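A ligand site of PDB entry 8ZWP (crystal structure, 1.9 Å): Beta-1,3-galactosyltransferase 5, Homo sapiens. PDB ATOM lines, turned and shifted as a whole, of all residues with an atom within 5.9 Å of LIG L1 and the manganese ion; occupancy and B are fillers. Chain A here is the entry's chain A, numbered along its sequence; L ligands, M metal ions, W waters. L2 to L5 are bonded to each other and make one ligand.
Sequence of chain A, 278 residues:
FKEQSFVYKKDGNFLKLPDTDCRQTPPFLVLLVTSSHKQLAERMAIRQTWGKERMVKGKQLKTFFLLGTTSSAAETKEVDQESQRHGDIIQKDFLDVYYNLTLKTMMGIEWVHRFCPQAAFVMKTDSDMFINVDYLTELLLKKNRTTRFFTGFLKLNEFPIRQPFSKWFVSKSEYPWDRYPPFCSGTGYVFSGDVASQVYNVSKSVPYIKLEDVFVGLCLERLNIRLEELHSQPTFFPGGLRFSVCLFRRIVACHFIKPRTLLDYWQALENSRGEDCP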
ATOM      1  N   VAL A  33       7.488  20.024   8.271  1.00  0.00           N
ATOM      2  CA  VAL A  33       8.164  20.722   7.177  1.00  0.00           C
ATOM      3  C   VAL A  33       7.368  21.974   6.827  1.00  0.00           C
ATOM      4  O   VAL A  33       6.179  21.891   6.521  1.00  0.00           O
ATOM      5  CB  VAL A  33       8.294  19.815   5.935  1.00  0.00           C
ATOM      6  CG1 VAL A  33       8.999  20.592   4.799  1.00  0.00           C
ATOM      7  CG2 VAL A  33       9.019  18.519   6.282  1.00  0.00           C
ATOM      8  N   THR A  34       8.030  23.125   6.850  1.00  0.00           N
ATOM      9  CA  THR A  34       7.397  24.357   6.415  1.00  0.00           C
ATOM     10  C   THR A  34       7.565  24.548   4.909  1.00  0.00           C
ATOM     11  O   THR A  34       8.636  24.270   4.342  1.00  0.00           O
ATOM     12  CB  THR A  34       7.977  25.570   7.152  1.00  0.00           C
ATOM     13  OG1 THR A  34       9.370  25.668   6.847  1.00  0.00           O
ATOM     14  CG2 THR A  34       7.777  25.412   8.659  1.00  0.00           C
ATOM     15  N   SER A  35       6.487  24.985   4.255  1.00  0.00           N
ATOM     16  CA  SER A  35       6.540  25.346   2.850  1.00  0.00           C
ATOM     17  C   SER A  35       5.306  26.189   2.551  1.00  0.00           C
ATOM     18  O   SER A  35       4.302  26.111   3.254  1.00  0.00           O
ATOM     19  CB  SER A  35       6.596  24.105   1.935  1.00  0.00           C
ATOM     20  OG  SER A  35       5.400  23.347   2.005  1.00  0.00           O
ATOM     21  N   SER A  36       5.402  27.007   1.502  1.00  0.00           N
ATOM     22  CA  SER A  36       4.261  27.814   1.101  1.00  0.00           C
ATOM     23  C   SER A  36       3.364  27.012   0.144  1.00  0.00           C
ATOM     24  O   SER A  36       3.752  25.948  -0.343  1.00  0.00           O
ATOM     25  CB  SER A  36       4.727  29.135   0.499  1.00  0.00           C
ATOM     26  OG  SER A  36       5.329  28.957  -0.762  1.00  0.00           O
ATOM     27  N   GLN A  39       4.663  25.793  -3.259  1.00  0.00           N
ATOM     28  CA  GLN A  39       5.848  24.929  -3.248  1.00  0.00           C
ATOM     29  C   GLN A  39       5.492  23.445  -3.265  1.00  0.00           C
ATOM     30  O   GLN A  39       6.079  22.662  -2.521  1.00  0.00           O
ATOM     31  CB  GLN A  39       6.733  25.267  -2.055  1.00  0.00           C
ATOM     32  CG  GLN A  39       7.335  26.658  -2.134  1.00  0.00           C
ATOM     33  CD  GLN A  39       8.322  26.944  -1.030  1.00  0.00           C
ATOM     34  OE1 GLN A  39       7.943  27.083   0.132  1.00  0.00           O
ATOM     35  NE2 GLN A  39       9.601  27.079  -1.379  1.00  0.00           N
ATOM     36  N   LEU A  66       3.402  21.780   7.201  1.00  0.00           N
ATOM     37  CA  LEU A  66       2.708  22.866   7.893  1.00  0.00           C
ATOM     38  C   LEU A  66       2.272  23.920   6.881  1.00  0.00           C
ATOM     39  O   LEU A  66       3.117  24.461   6.150  1.00  0.00           O
ATOM     40  CB  LEU A  66       3.632  23.480   8.944  1.00  0.00           C
ATOM     41  CG  LEU A  66       4.251  22.519   9.951  1.00  0.00           C
ATOM     42  CD1 LEU A  66       5.185  23.238  10.920  1.00  0.00           C
ATOM     43  CD2 LEU A  66       3.139  21.802  10.744  1.00  0.00           C
ATOM     44  N   ASP A  96      -0.533  32.647   5.203  1.00  0.00           N
ATOM     45  CA  ASP A  96       0.755  31.974   5.080  1.00  0.00           C
ATOM     46  C   ASP A  96       1.734  32.853   4.300  1.00  0.00           C
ATOM     47  O   ASP A  96       1.788  32.824   3.079  1.00  0.00           O
ATOM     48  CB  ASP A  96       0.544  30.614   4.424  1.00  0.00           C
ATOM     49  CG  ASP A  96       1.745  29.700   4.589  1.00  0.00           C
ATOM     50  OD1 ASP A  96       2.850  30.226   4.851  1.00  0.00           O
ATOM     51  OD2 ASP A  96       1.558  28.468   4.482  1.00  0.00           O
ATOM     52  N   VAL A  97       2.511  33.675   5.031  1.00  0.00           N
ATOM     53  CA  VAL A  97       3.538  34.530   4.441  1.00  0.00           C
ATOM     54  C   VAL A  97       4.792  34.485   5.314  1.00  0.00           C
ATOM     55  O   VAL A  97       4.742  34.053   6.464  1.00  0.00           O
ATOM     56  CB  VAL A  97       3.074  35.994   4.306  1.00  0.00           C
ATOM     57  CG1 VAL A  97       1.934  36.094   3.319  1.00  0.00           C
ATOM     58  CG2 VAL A  97       2.675  36.526   5.678  1.00  0.00           C
ATOM     59  N   TYR A  98       5.922  34.947   4.757  1.00  0.00           N
ATOM     60  CA  TYR A  98       7.186  34.789   5.479  1.00  0.00           C
ATOM     61  C   TYR A  98       7.083  35.368   6.894  1.00  0.00           C
ATOM     62  O   TYR A  98       7.498  34.726   7.869  1.00  0.00           O
ATOM     63  CB  TYR A  98       8.372  35.428   4.735  1.00  0.00           C
ATOM     64  CG  TYR A  98       9.717  34.986   5.319  1.00  0.00           C
ATOM     65  CD1 TYR A  98      10.330  35.706   6.349  1.00  0.00           C
ATOM     66  CD2 TYR A  98      10.362  33.840   4.856  1.00  0.00           C
ATOM     67  CE1 TYR A  98      11.557  35.304   6.896  1.00  0.00           C
ATOM     68  CE2 TYR A  98      11.594  33.417   5.403  1.00  0.00           C
ATOM     69  CZ  TYR A  98      12.170  34.156   6.425  1.00  0.00           C
ATOM     70  OH  TYR A  98      13.370  33.767   6.973  1.00  0.00           O
ATOM     71  N   LEU A 101       5.763  33.178   9.804  1.00  0.00           N
ATOM     72  CA  LEU A 101       6.374  31.891  10.118  1.00  0.00           C
ATOM     73  C   LEU A 101       6.300  31.533  11.598  1.00  0.00           C
ATOM     74  O   LEU A 101       6.257  30.362  11.944  1.00  0.00           O
ATOM     75  CB  LEU A 101       7.830  31.902   9.623  1.00  0.00           C
ATOM     76  CG  LEU A 101       7.869  31.692   8.122  1.00  0.00           C
ATOM     77  CD1 LEU A 101       9.334  31.750   7.612  1.00  0.00           C
ATOM     78  CD2 LEU A 101       7.201  30.368   7.742  1.00  0.00           C
ATOM     79  N   LYS A 104       3.230  29.726  12.062  1.00  0.00           N
ATOM     80  CA  LYS A 104       3.337  28.406  11.457  1.00  0.00           C
ATOM     81  C   LYS A 104       4.047  27.451  12.407  1.00  0.00           C
ATOM     82  O   LYS A 104       3.571  26.333  12.658  1.00  0.00           O
ATOM     83  CB  LYS A 104       4.066  28.475  10.117  1.00  0.00           C
ATOM     84  CG  LYS A 104       4.102  27.117   9.426  1.00  0.00           C
ATOM     85  CD  LYS A 104       4.581  27.208   7.978  1.00  0.00           C
ATOM     86  CE  LYS A 104       3.511  27.828   7.073  1.00  0.00           C
ATOM     87  NZ  LYS A 104       3.773  27.505   5.625  1.00  0.00           N
ATOM     88  N   THR A 125      11.657  21.686  10.124  1.00  0.00           N
ATOM     89  CA  THR A 125      12.631  21.913   9.068  1.00  0.00           C
ATOM     90  C   THR A 125      12.055  22.727   7.911  1.00  0.00           C
ATOM     91  O   THR A 125      10.846  22.719   7.648  1.00  0.00           O
ATOM     92  CB  THR A 125      13.223  20.570   8.555  1.00  0.00           C
ATOM     93  OG1 THR A 125      14.301  20.839   7.646  1.00  0.00           O
ATOM     94  CG2 THR A 125      12.161  19.724   7.856  1.00  0.00           C
ATOM     95  N   ASP A 126      12.953  23.430   7.222  1.00  0.00           N
ATOM     96  CA  ASP A 126      12.689  24.103   5.959  1.00  0.00           C
ATOM     97  C   ASP A 126      12.449  23.067   4.856  1.00  0.00           C
ATOM     98  O   ASP A 126      12.795  21.893   4.968  1.00  0.00           O
ATOM     99  CB  ASP A 126      13.882  24.963   5.510  1.00  0.00           C
ATOM    100  CG  ASP A 126      13.877  26.419   6.007  1.00  0.00           C
ATOM    101  OD1 ASP A 126      13.285  26.749   7.047  1.00  0.00           O
ATOM    102  OD2 ASP A 126      14.543  27.256   5.314  1.00  0.00           O
ATOM    103  N   SER A 127      11.938  23.535   3.736  1.00  0.00           N
ATOM    104  CA  SER A 127      11.686  22.626   2.618  1.00  0.00           C
ATOM    105  C   SER A 127      12.867  22.527   1.651  1.00  0.00           C
ATOM    106  O   SER A 127      12.952  21.555   0.894  1.00  0.00           O
ATOM    107  CB  SER A 127      10.422  23.035   1.870  1.00  0.00           C
ATOM    108  OG  SER A 127      10.495  24.415   1.525  1.00  0.00           O
ATOM    109  N   ASP A 128      13.758  23.523   1.634  1.00  0.00           N
ATOM    110  CA  ASP A 128      14.929  23.479   0.740  1.00  0.00           C
ATOM    111  C   ASP A 128      16.107  22.824   1.476  1.00  0.00           C
ATOM    112  O   ASP A 128      17.192  23.374   1.620  1.00  0.00           O
ATOM    113  CB  ASP A 128      15.256  24.866   0.205  1.00  0.00           C
ATOM    114  CG  ASP A 128      15.452  25.918   1.295  1.00  0.00           C
ATOM    115  OD1 ASP A 128      14.933  25.776   2.411  1.00  0.00           O
ATOM    116  OD2 ASP A 128      16.111  26.935   0.998  1.00  0.00           O
ATOM    117  N   MET A 129      15.855  21.584   1.903  1.00  0.00           N
ATOM    118  CA  MET A 129      16.756  20.879   2.807  1.00  0.00           C
ATOM    119  C   MET A 129      16.972  19.436   2.349  1.00  0.00           C
ATOM    120  O   MET A 129      16.068  18.814   1.788  1.00  0.00           O
ATOM    121  CB  MET A 129      16.188  20.803   4.237  1.00  0.00           C
ATOM    122  CG  MET A 129      16.030  22.147   4.940  1.00  0.00           C
ATOM    123  SD  MET A 129      17.569  22.901   5.456  1.00  0.00           S
ATOM    124  CE  MET A 129      18.102  21.763   6.722  1.00  0.00           C
ATOM    125  N   LYS A 167      16.191  40.910   4.898  1.00  0.00           N
ATOM    126  CA  LYS A 167      15.089  39.980   5.102  1.00  0.00           C
ATOM    127  C   LYS A 167      14.801  39.714   6.584  1.00  0.00           C
ATOM    128  O   LYS A 167      13.642  39.502   6.963  1.00  0.00           O
ATOM    129  CB  LYS A 167      15.428  38.669   4.382  1.00  0.00           C
ATOM    130  CG  LYS A 167      14.441  37.536   4.579  1.00  0.00           C
ATOM    131  CD  LYS A 167      15.023  36.252   3.978  1.00  0.00           C
ATOM    132  CE  LYS A 167      14.021  35.110   3.985  1.00  0.00           C
ATOM    133  NZ  LYS A 167      12.881  35.322   3.050  1.00  0.00           N
ATOM    134  N   TRP A 168      15.827  39.766   7.419  1.00  0.00           N
ATOM    135  CA  TRP A 168      15.693  39.493   8.843  1.00  0.00           C
ATOM    136  C   TRP A 168      15.737  40.760   9.699  1.00  0.00           C
ATOM    137  O   TRP A 168      16.044  40.692  10.894  1.00  0.00           O
ATOM    138  CB  TRP A 168      16.770  38.511   9.266  1.00  0.00           C
ATOM    139  CG  TRP A 168      16.667  37.189   8.552  1.00  0.00           C
ATOM    140  CD1 TRP A 168      15.538  36.407   8.379  1.00  0.00           C
ATOM    141  CD2 TRP A 168      17.720  36.513   7.883  1.00  0.00           C
ATOM    142  NE1 TRP A 168      15.854  35.274   7.664  1.00  0.00           N
ATOM    143  CE2 TRP A 168      17.187  35.312   7.345  1.00  0.00           C
ATOM    144  CE3 TRP A 168      19.082  36.787   7.698  1.00  0.00           C
ATOM    145  CZ2 TRP A 168      17.968  34.411   6.628  1.00  0.00           C
ATOM    146  CZ3 TRP A 168      19.852  35.884   7.000  1.00  0.00           C
ATOM    147  CH2 TRP A 168      19.294  34.710   6.471  1.00  0.00           C
ATOM    148  N   THR A 187      16.422  26.664   9.917  1.00  0.00           N
ATOM    149  CA  THR A 187      16.500  25.743   8.789  1.00  0.00           C
ATOM    150  C   THR A 187      16.182  24.304   9.210  1.00  0.00           C
ATOM    151  O   THR A 187      15.669  23.518   8.401  1.00  0.00           O
ATOM    152  CB  THR A 187      17.875  25.812   8.105  1.00  0.00           C
ATOM    153  OG1 THR A 187      18.931  25.557   9.039  1.00  0.00           O
ATOM    154  CG2 THR A 187      18.073  27.193   7.429  1.00  0.00           C
ATOM    155  N   HIS A 255      21.203  22.748   4.064  1.00  0.00           N
ATOM    156  CA  HIS A 255      20.306  23.754   3.508  1.00  0.00           C
ATOM    157  C   HIS A 255      20.679  24.087   2.056  1.00  0.00           C
ATOM    158  O   HIS A 255      21.694  23.627   1.521  1.00  0.00           O
ATOM    159  CB  HIS A 255      20.357  24.984   4.427  1.00  0.00           C
ATOM    160  CG  HIS A 255      19.359  26.066   4.131  1.00  0.00           C
ATOM    161  ND1 HIS A 255      19.715  27.401   4.231  1.00  0.00           N
ATOM    162  CD2 HIS A 255      18.044  26.050   3.848  1.00  0.00           C
ATOM    163  CE1 HIS A 255      18.664  28.154   3.960  1.00  0.00           C
ATOM    164  NE2 HIS A 255      17.635  27.362   3.744  1.00  0.00           N
ATOM    165  N   PHE A 256      19.844  24.917   1.429  1.00  0.00           N
ATOM    166  CA  PHE A 256      20.120  25.432   0.085  1.00  0.00           C
ATOM    167  C   PHE A 256      20.042  24.331  -0.965  1.00  0.00           C
ATOM    168  O   PHE A 256      20.852  24.280  -1.888  1.00  0.00           O
ATOM    169  CB  PHE A 256      21.478  26.127   0.028  1.00  0.00           C
ATOM    170  CG  PHE A 256      21.525  27.434   0.802  1.00  0.00           C
ATOM    171  CD1 PHE A 256      20.471  28.329   0.697  1.00  0.00           C
ATOM    172  CD2 PHE A 256      22.570  27.729   1.642  1.00  0.00           C
ATOM    173  CE1 PHE A 256      20.498  29.532   1.388  1.00  0.00           C
ATOM    174  CE2 PHE A 256      22.604  28.953   2.353  1.00  0.00           C
ATOM    175  CZ  PHE A 256      21.563  29.832   2.213  1.00  0.00           C
HETATM  176  N1  LIG L   1       7.887  29.416   3.936  1.00  0.00           N
HETATM  177  C1  LIG L   1       6.546  29.164   4.218  1.00  0.00           C
HETATM  178  N2  LIG L   1       5.673  30.172   3.862  1.00  0.00           N
HETATM  179  C2  LIG L   1       6.021  31.379   3.268  1.00  0.00           C
HETATM  180  C3  LIG L   1       7.410  31.556   3.016  1.00  0.00           C
HETATM  181  C4  LIG L   1       8.289  30.590   3.344  1.00  0.00           C
HETATM  182  O1  LIG L   1       6.147  28.127   4.748  1.00  0.00           O
HETATM  183  O2  LIG L   1       5.130  32.197   3.001  1.00  0.00           O
HETATM  184  C5  LIG L   1       8.884  28.377   4.277  1.00  0.00           C
HETATM  185  C6  LIG L   1       9.796  28.016   3.111  1.00  0.00           C
HETATM  186  O3  LIG L   1       9.267  27.014   2.260  1.00  0.00           O
HETATM  187  C7  LIG L   1      11.022  27.493   3.872  1.00  0.00           C
HETATM  188  C8  LIG L   1      11.083  28.425   5.080  1.00  0.00           C
HETATM  189  O4  LIG L   1       9.734  28.908   5.288  1.00  0.00           O
HETATM  190  O5  LIG L   1      10.808  26.146   4.259  1.00  0.00           O
HETATM  191  C9  LIG L   1      12.010  29.600   4.926  1.00  0.00           C
HETATM  192  O6  LIG L   1      11.808  30.185   3.617  1.00  0.00           O
HETATM  193  P1  LIG L   1      13.007  30.299   2.589  1.00  0.00           P
HETATM  194  O7  LIG L   1      12.459  30.911   1.350  1.00  0.00           O
HETATM  195  O8  LIG L   1      13.707  28.946   2.420  1.00  0.00           O
HETATM  196  O9  LIG L   1      14.050  31.293   3.298  1.00  0.00           O
HETATM  197  P2  LIG L   1      15.629  31.176   3.252  1.00  0.00           P
HETATM  198  O10 LIG L   1      15.961  31.522   1.804  1.00  0.00           O
HETATM  199  O11 LIG L   1      16.089  32.316   4.161  1.00  0.00           O
HETATM  200  O12 LIG L   1      16.113  29.785   3.644  1.00  0.00           O
HETATM  201  C1  LG2 L   2      21.387  39.432   1.429  1.00  0.00           C
HETATM  202  C2  LG2 L   2      21.692  39.045   2.863  1.00  0.00           C
HETATM  203  C3  LG2 L   2      20.901  37.808   3.275  1.00  0.00           C
HETATM  204  C4  LG2 L   2      21.079  36.679   2.249  1.00  0.00           C
HETATM  205  C5  LG2 L   2      20.149  35.506   2.505  1.00  0.00           C
HETATM  206  C6  LG2 L   2      21.605  38.237   0.502  1.00  0.00           C
HETATM  207  O1  LG2 L   2      21.265  38.606  -0.805  1.00  0.00           O
HETATM  208  O2  LG2 L   2      22.227  40.515   1.020  1.00  0.00           O
HETATM  209  O3  LG2 L   2      21.402  40.138   3.734  1.00  0.00           O
HETATM  210  O4  LG2 L   2      21.281  37.356   4.570  1.00  0.00           O
HETATM  211  O5  LG2 L   2      20.782  37.149   0.926  1.00  0.00           O
HETATM  212  O6  LG2 L   2      18.916  35.673   1.828  1.00  0.00           O
HETATM  213  C1  LG3 L   3      22.684  37.002   4.720  1.00  0.00           C
HETATM  214  C2  LG3 L   3      23.176  37.715   5.996  1.00  0.00           C
HETATM  215  C3  LG3 L   3      24.591  37.334   6.378  1.00  0.00           C
HETATM  216  C4  LG3 L   3      24.592  35.849   6.640  1.00  0.00           C
HETATM  217  C5  LG3 L   3      24.113  35.098   5.378  1.00  0.00           C
HETATM  218  C6  LG3 L   3      23.913  33.557   5.604  1.00  0.00           C
HETATM  219  O1  LG3 L   3      23.141  39.136   5.857  1.00  0.00           O
HETATM  220  O2  LG3 L   3      25.001  37.989   7.596  1.00  0.00           O
HETATM  221  O3  LG3 L   3      23.673  35.553   7.715  1.00  0.00           O
HETATM  222  O4  LG3 L   3      22.871  35.578   4.784  1.00  0.00           O
HETATM  223  O5  LG3 L   3      22.565  33.138   5.447  1.00  0.00           O
HETATM  224  C1  LG4 L   4      24.238  34.882   8.849  1.00  0.00           C
HETATM  225  C2  LG4 L   4      23.189  33.930   9.417  1.00  0.00           C
HETATM  226  C3  LG4 L   4      22.060  34.684  10.061  1.00  0.00           C
HETATM  227  C4  LG4 L   4      22.624  35.599  11.109  1.00  0.00           C
HETATM  228  C5  LG4 L   4      23.624  36.591  10.528  1.00  0.00           C
HETATM  229  C6  LG4 L   4      24.257  37.444  11.588  1.00  0.00           C
HETATM  230  O1  LG4 L   4      22.635  33.113   8.369  1.00  0.00           O
HETATM  231  O2  LG4 L   4      21.134  33.766  10.686  1.00  0.00           O
HETATM  232  O3  LG4 L   4      23.345  34.789  12.040  1.00  0.00           O
HETATM  233  O4  LG4 L   4      24.737  35.869   9.858  1.00  0.00           O
HETATM  234  O5  LG4 L   4      25.119  38.360  10.932  1.00  0.00           O
HETATM  235  C1  LG5 L   5      19.777  34.248  10.626  1.00  0.00           C
HETATM  236  C2  LG5 L   5      18.836  33.054  10.570  1.00  0.00           C
HETATM  237  C3  LG5 L   5      17.394  33.542  10.591  1.00  0.00           C
HETATM  238  C4  LG5 L   5      17.139  34.514  11.753  1.00  0.00           C
HETATM  239  C5  LG5 L   5      18.207  35.607  11.737  1.00  0.00           C
HETATM  240  C6  LG5 L   5      18.072  36.576  12.921  1.00  0.00           C
HETATM  241  C7  LG5 L   5      19.683  31.070   9.356  1.00  0.00           C
HETATM  242  C8  LG5 L   5      20.281  30.604   8.043  1.00  0.00           C
HETATM  243  N1  LG5 L   5      19.055  32.256   9.353  1.00  0.00           N
HETATM  244  O1  LG5 L   5      16.484  32.438  10.685  1.00  0.00           O
HETATM  245  O2  LG5 L   5      17.139  33.849  12.997  1.00  0.00           O
HETATM  246  O3  LG5 L   5      19.501  35.041  11.779  1.00  0.00           O
HETATM  247  O4  LG5 L   5      18.991  37.637  12.709  1.00  0.00           O
HETATM  248  O5  LG5 L   5      19.771  30.348  10.334  1.00  0.00           O
HETATM  249 MN    MN M   1      15.484  27.859   3.271  1.00  0.00          MN
HETATM  250  O   HOH W   1      14.263  31.398   6.366  1.00  0.00           O
HETATM  251  O   HOH W   2      13.467  28.292  -0.069  1.00  0.00           O
HETATM  252  O   HOH W   3      16.738  29.550   0.181  1.00  0.00           O
HETATM  253  O   HOH W   4       3.812  32.682   0.868  1.00  0.00           O
HETATM  254  O   HOH W   5      17.706  30.798   5.966  1.00  0.00           O
HETATM  255  O   HOH W   6      10.403  29.989   0.152  1.00  0.00           O
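The backbone carbonyl oxygen of Asp 128 sits at hydrogen-bond distance from the backbone NH of Phe 256 (3.1 Å).
The backbone NH (N) of Asp 126 lies within hydrogen-bond range of the backbone carbonyl oxygen (O) of Thr 187 (3.0 Å).
NZ of Lys 104 lies within salt-bridge range of OD2 of Asp 96 (2.7 Å).
The side-chain amino group of Lys 104 is in hydrogen-bond range of the backbone carbonyl oxygen of Ser 35 (2.8 Å).
The side-chain amino group of Lys 104 is in hydrogen-bond range of the backbone carbonyl oxygen of Leu 66, 3.2 Å away.
The backbone carbonyl oxygen (O) of Thr 34 lies close to the side-chain hydroxyl (OG) of Ser 127 (3.4 Å).
N of Thr 34 is in hydrogen-bond range of O of Thr 125, 3.0 Å away.
The indole nitrogen (NE1) of Trp 168 lies within hydrogen-bond range of the side-chain hydroxyl (OH) of Tyr 98, at 3.0 Å.
OE1 of Gln 39 sits at hydrogen-bond distance from O3 of LIG L1, at 2.5 Å.
The side-chain amino group of Lys 104 lies within hydrogen-bond range of an oxygen (O1) of LIG L1, at 2.6 Å.
O of Thr 34 sits at hydrogen-bond distance from O5 of LIG L1.
OG1 of Thr 34 sits at hydrogen-bond distance from O5 of LIG L1 (3.0 Å).
N of Ser 127 lies within hydrogen-bond range of O5 of LIG L1 (2.9 Å).
An oxygen (O3) of LIG L1 lies within hydrogen-bond range of the side-chain hydroxyl (OG) of Ser 127 (3.0 Å).
A nitrogen (N2) of LIG L1 sits at hydrogen-bond distance from the side-chain carboxylate (OD1) of Asp 96, 3.0 Å away.
N of Ser 35 sits close to O1 of LIG L1 (3.2 Å).
An oxygen (O2) of LIG L1 is in hydrogen-bond range of the backbone NH of Tyr 98 (3.4 Å).
O12 of LIG L1 is bound to the manganese ion, 2.1 Å away.
The manganese ion is bound by an oxygen (O8) of LIG L1.
The manganese ion is bound by NE2 of His 255 (2.3 Å).
The manganese ion is bound by the side-chain carboxylate (OD1) of Asp 128, 2.3 Å away.
The side-chain carboxylate (OD2) of Asp 126 is bound to the manganese ion (2.3 Å).
The manganese ion is bound by OD2 of Asp 128 (2.5 Å).
The manganese ion has six donor atoms within binding distance.
Water W6 lies within hydrogen-bond range of an oxygen (O7) of LIG L1 and the side-chain amide nitrogen of Gln 39.
Water W4 bridges O2 of LIG L1 (2.6 Å) and O of Asp 96 (3.0 Å).
Water W1 lies within hydrogen-bond range of OH of Tyr 98 (2.6 Å) and O11 of LIG L1 (3.0 Å).
Ser 36 touches LIG L1.
Val 97 touches LIG L1.
Leu 101 touches LIG L1.
CE of Lys 167 touches O11 of LIG L1, at 3.5 Å.
CZ2 of Trp 168 touches O11 of LIG L1 (3.7 Å).
Hydrophobic or aromatic side chains within 4 Å of LIG L1: Tyr 98, Leu 101, Trp 168 and His 255.
15 residues have an atom within 4 Å of LIG L1: Thr 34, Ser 35, Ser 36, Gln 39, Asp 96, Val 97, Tyr 98, Leu 101, Lys 104, Asp 126, Ser 127, Asp 128, Lys 167, Trp 168 and His 255.
The nearest printed residue that does not touch LIG L1 is Thr 125 (4.8 Å).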
